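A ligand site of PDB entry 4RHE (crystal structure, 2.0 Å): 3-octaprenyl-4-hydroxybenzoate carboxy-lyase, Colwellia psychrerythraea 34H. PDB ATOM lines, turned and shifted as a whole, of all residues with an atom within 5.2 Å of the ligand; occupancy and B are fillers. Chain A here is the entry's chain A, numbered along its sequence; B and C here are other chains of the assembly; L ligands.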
ATOM      1  N   THR A  17      24.490   3.721  -2.232  1.00  0.00           N
ATOM      2  CA  THR A  17      24.090   4.735  -3.211  1.00  0.00           C
ATOM      3  C   THR A  17      22.788   4.336  -3.871  1.00  0.00           C
ATOM      4  O   THR A  17      22.215   3.249  -3.573  1.00  0.00           O
ATOM      5  CB  THR A  17      25.171   5.032  -4.267  1.00  0.00           C
ATOM      6  OG1 THR A  17      25.449   3.843  -5.012  1.00  0.00           O
ATOM      7  CG2 THR A  17      26.433   5.482  -3.609  1.00  0.00           C
ATOM      8  N   GLY A  18      22.368   5.221  -4.767  1.00  0.00           N
ATOM      9  CA  GLY A  18      21.090   5.191  -5.357  1.00  0.00           C
ATOM     10  C   GLY A  18      20.831   4.175  -6.423  1.00  0.00           C
ATOM     11  O   GLY A  18      20.082   4.433  -7.307  1.00  0.00           O
ATOM     12  N   ALA A  19      21.455   3.024  -6.362  1.00  0.00           N
ATOM     13  CA  ALA A  19      21.125   1.959  -7.288  1.00  0.00           C
ATOM     14  C   ALA A  19      20.162   1.021  -6.612  1.00  0.00           C
ATOM     15  O   ALA A  19      20.072   0.954  -5.337  1.00  0.00           O
ATOM     16  CB  ALA A  19      22.376   1.237  -7.749  1.00  0.00           C
ATOM     17  N   SER A  20      19.412   0.301  -7.431  1.00  0.00           N
ATOM     18  CA  SER A  20      18.496  -0.653  -6.861  1.00  0.00           C
ATOM     19  C   SER A  20      19.356  -1.757  -6.249  1.00  0.00           C
ATOM     20  O   SER A  20      20.523  -1.960  -6.613  1.00  0.00           O
ATOM     21  CB  SER A  20      17.562  -1.119  -7.975  1.00  0.00           C
ATOM     22  OG  SER A  20      16.584  -2.052  -7.588  1.00  0.00           O
ATOM     23  N   SER A  44      24.080   8.244   0.423  1.00  0.00           N
ATOM     24  CA  SER A  44      23.757   9.448  -0.366  1.00  0.00           C
ATOM     25  C   SER A  44      22.275   9.635  -0.238  1.00  0.00           C
ATOM     26  O   SER A  44      21.589   8.756   0.311  1.00  0.00           O
ATOM     27  CB  SER A  44      24.109   9.243  -1.852  1.00  0.00           C
ATOM     28  OG  SER A  44      23.326   8.208  -2.440  1.00  0.00           O
ATOM     29  N   ALA A  46      20.172   9.855  -2.723  1.00  0.00           N
ATOM     30  CA  ALA A  46      19.493   8.872  -3.539  1.00  0.00           C
ATOM     31  C   ALA A  46      19.524   7.490  -2.889  1.00  0.00           C
ATOM     32  O   ALA A  46      18.562   6.769  -2.946  1.00  0.00           O
ATOM     33  CB  ALA A  46      20.066   8.793  -4.927  1.00  0.00           C
ATOM     34  N   GLY A  47      20.600   7.149  -2.239  1.00  0.00           N
ATOM     35  CA  GLY A  47      20.602   5.919  -1.423  1.00  0.00           C
ATOM     36  C   GLY A  47      19.498   5.835  -0.347  1.00  0.00           C
ATOM     37  O   GLY A  47      18.925   4.757  -0.140  1.00  0.00           O
ATOM     38  N   ILE A  49      16.476   7.279  -0.551  1.00  0.00           N
ATOM     39  CA  ILE A  49      15.292   7.078  -1.272  1.00  0.00           C
ATOM     40  C   ILE A  49      15.142   5.627  -1.679  1.00  0.00           C
ATOM     41  O   ILE A  49      14.061   5.053  -1.582  1.00  0.00           O
ATOM     42  CB  ILE A  49      15.215   8.014  -2.499  1.00  0.00           C
ATOM     43  CG1 ILE A  49      15.202   9.477  -2.073  1.00  0.00           C
ATOM     44  CG2 ILE A  49      14.015   7.683  -3.334  1.00  0.00           C
ATOM     45  CD1 ILE A  49      15.533  10.391  -3.223  1.00  0.00           C
ATOM     46  N   VAL A  50      16.208   5.014  -2.170  1.00  0.00           N
ATOM     47  CA  VAL A  50      16.124   3.618  -2.488  1.00  0.00           C
ATOM     48  C   VAL A  50      15.856   2.717  -1.284  1.00  0.00           C
ATOM     49  O   VAL A  50      15.069   1.750  -1.376  1.00  0.00           O
ATOM     50  CB  VAL A  50      17.409   3.167  -3.264  1.00  0.00           C
ATOM     51  CG1 VAL A  50      17.413   1.676  -3.525  1.00  0.00           C
ATOM     52  CG2 VAL A  50      17.468   3.900  -4.584  1.00  0.00           C
ATOM     53  N   THR A  53      12.114   3.042  -0.266  1.00  0.00           N
ATOM     54  CA  THR A  53      11.137   2.417  -1.175  1.00  0.00           C
ATOM     55  C   THR A  53      11.299   0.901  -1.347  1.00  0.00           C
ATOM     56  O   THR A  53      10.314   0.178  -1.468  1.00  0.00           O
ATOM     57  CB  THR A  53      11.058   3.127  -2.526  1.00  0.00           C
ATOM     58  OG1 THR A  53      12.311   3.108  -3.186  1.00  0.00           O
ATOM     59  CG2 THR A  53      10.706   4.611  -2.347  1.00  0.00           C
ATOM     60  N   GLU A  54      12.519   0.403  -1.355  1.00  0.00           N
ATOM     61  CA  GLU A  54      12.701  -0.981  -1.672  1.00  0.00           C
ATOM     62  C   GLU A  54      12.517  -1.872  -0.470  1.00  0.00           C
ATOM     63  O   GLU A  54      11.964  -2.936  -0.607  1.00  0.00           O
ATOM     64  CB  GLU A  54      14.098  -1.275  -2.241  1.00  0.00           C
ATOM     65  CG  GLU A  54      14.174  -0.753  -3.664  1.00  0.00           C
ATOM     66  CD  GLU A  54      15.380  -1.266  -4.472  1.00  0.00           C
ATOM     67  OE1 GLU A  54      16.252  -2.025  -3.942  1.00  0.00           O
ATOM     68  OE2 GLU A  54      15.394  -0.842  -5.657  1.00  0.00           O
ATOM     69  N   CYS A 108      25.979   0.210  -5.880  1.00  0.00           N
ATOM     70  CA  CYS A 108      26.738   1.287  -6.437  1.00  0.00           C
ATOM     71  C   CYS A 108      26.014   1.778  -7.683  1.00  0.00           C
ATOM     72  O   CYS A 108      25.761   0.991  -8.617  1.00  0.00           O
ATOM     73  CB  CYS A 108      28.122   0.784  -6.795  1.00  0.00           C
ATOM     74  SG  CYS A 108      29.221   2.062  -7.440  1.00  0.00           S
ATOM     75  N   SER A 109      25.652   3.022  -7.739  1.00  0.00           N
ATOM     76  CA  SER A 109      25.032   3.505  -8.960  1.00  0.00           C
ATOM     77  C   SER A 109      26.064   3.622 -10.065  1.00  0.00           C
ATOM     78  O   SER A 109      27.235   3.808  -9.778  1.00  0.00           O
ATOM     79  CB  SER A 109      24.439   4.908  -8.789  1.00  0.00           C
ATOM     80  OG  SER A 109      25.455   5.748  -8.262  1.00  0.00           O
ATOM     81  N   THR A 110      25.610   3.645 -11.314  1.00  0.00           N
ATOM     82  CA  THR A 110      26.539   3.975 -12.356  1.00  0.00           C
ATOM     83  C   THR A 110      27.070   5.406 -12.252  1.00  0.00           C
ATOM     84  O   THR A 110      28.205   5.592 -12.645  1.00  0.00           O
ATOM     85  CB  THR A 110      26.056   3.673 -13.784  1.00  0.00           C
ATOM     86  OG1 THR A 110      25.020   4.594 -14.139  1.00  0.00           O
ATOM     87  CG2 THR A 110      25.587   2.241 -13.863  1.00  0.00           C
ATOM     88  N   GLY A 111      26.309   6.363 -11.699  1.00  0.00           N
ATOM     89  CA  GLY A 111      26.787   7.754 -11.528  1.00  0.00           C
ATOM     90  C   GLY A 111      27.846   7.927 -10.463  1.00  0.00           C
ATOM     91  O   GLY A 111      28.798   8.624 -10.643  1.00  0.00           O
ATOM     92  N   THR A 112      27.746   7.157  -9.374  1.00  0.00           N
ATOM     93  CA  THR A 112      28.821   7.117  -8.351  1.00  0.00           C
ATOM     94  C   THR A 112      30.034   6.353  -8.883  1.00  0.00           C
ATOM     95  O   THR A 112      31.142   6.763  -8.630  1.00  0.00           O
ATOM     96  CB  THR A 112      28.292   6.596  -7.011  1.00  0.00           C
ATOM     97  OG1 THR A 112      27.512   7.632  -6.436  1.00  0.00           O
ATOM     98  CG2 THR A 112      29.440   6.161  -6.019  1.00  0.00           C
ATOM     99  N   ARG A 144      24.760  -2.134 -10.009  1.00  0.00           N
ATOM    100  CA  ARG A 144      23.495  -2.696 -10.382  1.00  0.00           C
ATOM    101  C   ARG A 144      22.965  -1.788 -11.445  1.00  0.00           C
ATOM    102  O   ARG A 144      22.613  -0.636 -11.184  1.00  0.00           O
ATOM    103  CB  ARG A 144      22.593  -2.708  -9.133  1.00  0.00           C
ATOM    104  CG  ARG A 144      21.405  -3.640  -9.104  1.00  0.00           C
ATOM    105  CD  ARG A 144      20.566  -3.817 -10.359  1.00  0.00           C
ATOM    106  NE  ARG A 144      19.864  -2.634 -10.773  1.00  0.00           N
ATOM    107  CZ  ARG A 144      19.217  -2.514 -11.921  1.00  0.00           C
ATOM    108  NH1 ARG A 144      19.185  -3.534 -12.791  1.00  0.00           N
ATOM    109  NH2 ARG A 144      18.646  -1.349 -12.228  1.00  0.00           N
ATOM    110  N   GLU A 145      23.016  -2.295 -12.678  1.00  0.00           N
ATOM    111  CA  GLU A 145      22.425  -1.654 -13.843  1.00  0.00           C
ATOM    112  C   GLU A 145      22.428  -2.653 -14.983  1.00  0.00           C
ATOM    113  O   GLU A 145      23.339  -3.483 -15.094  1.00  0.00           O
ATOM    114  CB  GLU A 145      23.240  -0.422 -14.292  1.00  0.00           C
ATOM    115  CG  GLU A 145      22.572   0.409 -15.403  1.00  0.00           C
ATOM    116  CD  GLU A 145      21.154   0.888 -15.017  1.00  0.00           C
ATOM    117  OE1 GLU A 145      20.958   2.023 -14.394  1.00  0.00           O
ATOM    118  OE2 GLU A 145      20.211   0.119 -15.407  1.00  0.00           O
ATOM    119  N   TRP B  89      13.125  11.546  -9.083  1.00  0.00           N
ATOM    120  CA  TRP B  89      13.279  10.168  -9.575  1.00  0.00           C
ATOM    121  C   TRP B  89      12.010   9.386  -9.955  1.00  0.00           C
ATOM    122  O   TRP B  89      12.158   8.435 -10.715  1.00  0.00           O
ATOM    123  CB  TRP B  89      14.102   9.342  -8.599  1.00  0.00           C
ATOM    124  CG  TRP B  89      15.349  10.064  -8.177  1.00  0.00           C
ATOM    125  CD1 TRP B  89      15.674  10.486  -6.916  1.00  0.00           C
ATOM    126  CD2 TRP B  89      16.410  10.536  -9.047  1.00  0.00           C
ATOM    127  NE1 TRP B  89      16.879  11.189  -6.952  1.00  0.00           N
ATOM    128  CE2 TRP B  89      17.331  11.222  -8.249  1.00  0.00           C
ATOM    129  CE3 TRP B  89      16.660  10.402 -10.438  1.00  0.00           C
ATOM    130  CZ2 TRP B  89      18.529  11.772  -8.766  1.00  0.00           C
ATOM    131  CZ3 TRP B  89      17.814  10.945 -10.959  1.00  0.00           C
ATOM    132  CH2 TRP B  89      18.737  11.628 -10.124  1.00  0.00           C
ATOM    133  N   SER B 121      25.521  11.253 -14.276  1.00  0.00           N
ATOM    134  CA  SER B 121      24.205  10.893 -13.823  1.00  0.00           C
ATOM    135  C   SER B 121      23.891  11.529 -12.454  1.00  0.00           C
ATOM    136  O   SER B 121      23.483  10.813 -11.558  1.00  0.00           O
ATOM    137  CB  SER B 121      24.082   9.360 -13.744  1.00  0.00           C
ATOM    138  OG  SER B 121      22.739   8.881 -13.747  1.00  0.00           O
ATOM    139  N   ASP B 122      24.094  12.855 -12.298  1.00  0.00           N
ATOM    140  CA  ASP B 122      24.042  13.507 -10.940  1.00  0.00           C
ATOM    141  C   ASP B 122      22.707  14.153 -10.646  1.00  0.00           C
ATOM    142  O   ASP B 122      22.464  14.556  -9.522  1.00  0.00           O
ATOM    143  CB  ASP B 122      25.138  14.569 -10.766  1.00  0.00           C
ATOM    144  CG  ASP B 122      26.440  13.986 -10.221  1.00  0.00           C
ATOM    145  OD1 ASP B 122      26.371  13.063  -9.323  1.00  0.00           O
ATOM    146  OD2 ASP B 122      27.534  14.412 -10.712  1.00  0.00           O
ATOM    147  N   ASN B 123      21.868  14.256 -11.674  1.00  0.00           N
ATOM    148  CA  ASN B 123      20.564  14.895 -11.594  1.00  0.00           C
ATOM    149  C   ASN B 123      19.720  14.241 -12.695  1.00  0.00           C
ATOM    150  O   ASN B 123      20.206  13.385 -13.444  1.00  0.00           O
ATOM    151  CB  ASN B 123      20.698  16.399 -11.880  1.00  0.00           C
ATOM    152  CG  ASN B 123      21.310  16.678 -13.245  1.00  0.00           C
ATOM    153  OD1 ASN B 123      21.048  16.025 -14.227  1.00  0.00           O
ATOM    154  ND2 ASN B 123      22.108  17.678 -13.310  1.00  0.00           N
ATOM    155  N   ARG B 127      20.759  11.641 -15.652  1.00  0.00           N
ATOM    156  CA  ARG B 127      20.276  10.264 -15.537  1.00  0.00           C
ATOM    157  C   ARG B 127      19.420   9.923 -16.753  1.00  0.00           C
ATOM    158  O   ARG B 127      19.521   8.823 -17.288  1.00  0.00           O
ATOM    159  CB  ARG B 127      19.519  10.052 -14.204  1.00  0.00           C
ATOM    160  CG  ARG B 127      18.654   8.827 -14.142  1.00  0.00           C
ATOM    161  CD  ARG B 127      19.479   7.541 -14.274  1.00  0.00           C
ATOM    162  NE  ARG B 127      18.689   6.363 -14.097  1.00  0.00           N
ATOM    163  CZ  ARG B 127      19.162   5.115 -14.118  1.00  0.00           C
ATOM    164  NH1 ARG B 127      20.434   4.863 -14.383  1.00  0.00           N
ATOM    165  NH2 ARG B 127      18.329   4.098 -13.968  1.00  0.00           N
ATOM    166  N   TYR C 174      13.238  -2.488  -7.655  1.00  0.00           N
ATOM    167  CA  TYR C 174      12.363  -1.322  -7.435  1.00  0.00           C
ATOM    168  C   TYR C 174      10.879  -1.600  -7.755  1.00  0.00           C
ATOM    169  O   TYR C 174      10.013  -0.861  -7.377  1.00  0.00           O
ATOM    170  CB  TYR C 174      12.814  -0.092  -8.230  1.00  0.00           C
ATOM    171  CG  TYR C 174      13.081  -0.323  -9.681  1.00  0.00           C
ATOM    172  CD1 TYR C 174      12.042  -0.332 -10.592  1.00  0.00           C
ATOM    173  CD2 TYR C 174      14.387  -0.555 -10.154  1.00  0.00           C
ATOM    174  CE1 TYR C 174      12.292  -0.536 -11.943  1.00  0.00           C
ATOM    175  CE2 TYR C 174      14.646  -0.750 -11.513  1.00  0.00           C
ATOM    176  CZ  TYR C 174      13.555  -0.707 -12.398  1.00  0.00           C
ATOM    177  OH  TYR C 174      13.685  -0.888 -13.765  1.00  0.00           O
ATOM    178  N   TYR C 207      10.083   4.195 -11.202  1.00  0.00           N
ATOM    179  CA  TYR C 207      10.325   4.270  -9.758  1.00  0.00           C
ATOM    180  C   TYR C 207       9.158   4.902  -8.948  1.00  0.00           C
ATOM    181  O   TYR C 207       8.601   5.941  -9.347  1.00  0.00           O
ATOM    182  CB  TYR C 207      11.578   5.085  -9.549  1.00  0.00           C
ATOM    183  CG  TYR C 207      12.792   4.627 -10.343  1.00  0.00           C
ATOM    184  CD1 TYR C 207      12.979   3.292 -10.654  1.00  0.00           C
ATOM    185  CD2 TYR C 207      13.786   5.530 -10.682  1.00  0.00           C
ATOM    186  CE1 TYR C 207      14.121   2.872 -11.357  1.00  0.00           C
ATOM    187  CE2 TYR C 207      14.926   5.133 -11.362  1.00  0.00           C
ATOM    188  CZ  TYR C 207      15.092   3.802 -11.704  1.00  0.00           C
ATOM    189  OH  TYR C 207      16.207   3.421 -12.370  1.00  0.00           O
HETATM  190  N1  LIG L   1      20.909   4.231 -10.993  1.00  0.00           N
HETATM  191  C1  LIG L   1      21.666   3.158 -11.355  1.00  0.00           C
HETATM  192  O1  LIG L   1      22.762   3.437 -11.909  1.00  0.00           O
HETATM  193  N2  LIG L   1      21.275   1.826 -11.133  1.00  0.00           N
HETATM  194  C2  LIG L   1      20.146   1.490 -10.485  1.00  0.00           C
HETATM  195  O2  LIG L   1      19.695   0.348 -10.191  1.00  0.00           O
HETATM  196  C3  LIG L   1      19.307   2.588 -10.057  1.00  0.00           C
HETATM  197  N3  LIG L   1      18.168   2.284  -9.412  1.00  0.00           N
HETATM  198  C4  LIG L   1      17.332   3.255  -8.924  1.00  0.00           C
HETATM  199  C5  LIG L   1      16.168   2.909  -8.221  1.00  0.00           C
HETATM  200  C6  LIG L   1      15.307   3.864  -7.714  1.00  0.00           C
HETATM  201  C7  LIG L   1      14.060   3.406  -6.988  1.00  0.00           C
HETATM  202  C8  LIG L   1      15.641   5.314  -7.935  1.00  0.00           C
HETATM  203  C9  LIG L   1      14.728   6.406  -7.414  1.00  0.00           C
HETATM  204  C10 LIG L   1      16.794   5.678  -8.643  1.00  0.00           C
HETATM  205  C11 LIG L   1      17.692   4.698  -9.163  1.00  0.00           C
HETATM  206  N4  LIG L   1      18.913   5.010  -9.879  1.00  0.00           N
HETATM  207  C12 LIG L   1      19.743   3.973 -10.340  1.00  0.00           C
HETATM  208  C13 LIG L   1      19.378   6.386 -10.229  1.00  0.00           C
HETATM  209  C14 LIG L   1      20.335   6.981  -9.223  1.00  0.00           C
HETATM  210  O3  LIG L   1      19.628   6.997  -7.966  1.00  0.00           O
HETATM  211  C15 LIG L   1      20.642   8.378  -9.755  1.00  0.00           C
HETATM  212  O4  LIG L   1      21.407   8.396 -11.004  1.00  0.00           O
HETATM  213  C16 LIG L   1      21.339   9.231  -8.714  1.00  0.00           C
HETATM  214  O5  LIG L   1      21.723  10.434  -9.394  1.00  0.00           O
HETATM  215  C17 LIG L   1      22.553   8.517  -8.096  1.00  0.00           C
HETATM  216  O6  LIG L   1      23.134   9.429  -7.153  1.00  0.00           O
HETATM  217  P1  LIG L   1      24.133   8.793  -6.098  1.00  0.00           P
HETATM  218  O7  LIG L   1      23.492   7.910  -5.115  1.00  0.00           O
HETATM  219  O8  LIG L   1      25.116   8.150  -7.098  1.00  0.00           O
HETATM  220  O9  LIG L   1      24.692  10.016  -5.423  1.00  0.00           O
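The side-chain hydroxyl of Thr 110 sits at hydrogen-bond distance from an oxygen (O1) of the ligand (3.4 Å). The side-chain hydroxyl (OG) of Ser 109 is in hydrogen-bond range of an oxygen (O8) of the ligand (2.7 Å). OG of Ser 44 sits at hydrogen-bond distance from O7 of the ligand (2.7 Å). N of Ser 20 is in hydrogen-bond range of O2 of the ligand (2.8 Å). The side-chain carboxylate of Glu 145 is in hydrogen-bond range of a nitrogen (N2) of the ligand, at 3.3 Å. NH1 of Arg 127 of chain B is in hydrogen-bond range of N1 of the ligand. An oxygen (O3) of the ligand is in hydrogen-bond range of the backbone carbonyl oxygen (O) of Gly 18. OG1 of Thr 112 sits at hydrogen-bond distance from O8 of the ligand, 2.5 Å away. An oxygen (O1) of the ligand lies within hydrogen-bond range of the backbone NH (N) of Thr 110, 2.9 Å away. N of Gly 18 is in hydrogen-bond range of O7 of the ligand (2.9 Å). OG of Ser 121 of chain B is in hydrogen-bond range of O4 of the ligand (3.1 Å). O of Ser 121 of chain B sits at hydrogen-bond distance from O5 of the ligand. The backbone carbonyl oxygen (O) of Arg 144 is in hydrogen-bond range of a nitrogen (N2) of the ligand (2.8 Å). The guanidinium group of Arg 144 is in hydrogen-bond range of an oxygen (O2) of the ligand (2.9 Å).
The side-chain carboxylate of Glu 145 is in salt-bridge range of the guanidinium group of Arg 127 of chain B (2.9 Å). OE2 of Glu 54 lies within hydrogen-bond range of N of Tyr 174 of chain C, 3.4 Å away. The side-chain hydroxyl (OG) of Ser 20 lies within hydrogen-bond range of the side-chain carboxylate (OE2) of Glu 54 (2.6 Å). The guanidinium group (NH2) of Arg 127 of chain B sits at hydrogen-bond distance from the side-chain hydroxyl (OH) of Tyr 207 of chain C, 2.7 Å away. The side-chain carboxylate of Glu 145 lies within salt-bridge range of the guanidinium group of Arg 144 (3.8 Å). OG1 of Thr 17 is in hydrogen-bond range of N of Ser 109 (2.9 Å). The backbone NH of Thr 112 is in hydrogen-bond range of the side-chain hydroxyl of Ser 109 (2.9 Å). The side-chain hydroxyl of Ser 44 sits at hydrogen-bond distance from the backbone NH of Gly 47.
Residues that only touch the ligand: Trp 89 of chain B (3.2 Å), Tyr 207 of chain C (3.3 Å), Ala 19 (3.4 Å), Thr 17 (3.4 Å), Ala 46 (3.5 Å), Val 50 (3.8 Å) and Tyr 174 of chain C (3.9 Å). 17 residues have an atom within 4 Å of the ligand: Thr 17, Gly 18, Ala 19, Ser 20, Ser 44, Ala 46, Val 50, Ser 109, Thr 110, Thr 112, Arg 144, Glu 145, Trp 89 of chain B, Ser 121 of chain B, Arg 127 of chain B, Tyr 174 of chain C and Tyr 207 of chain C. The nearest printed residue that does not touch the ligand is Asp 122 of chain B (4.05 Å).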
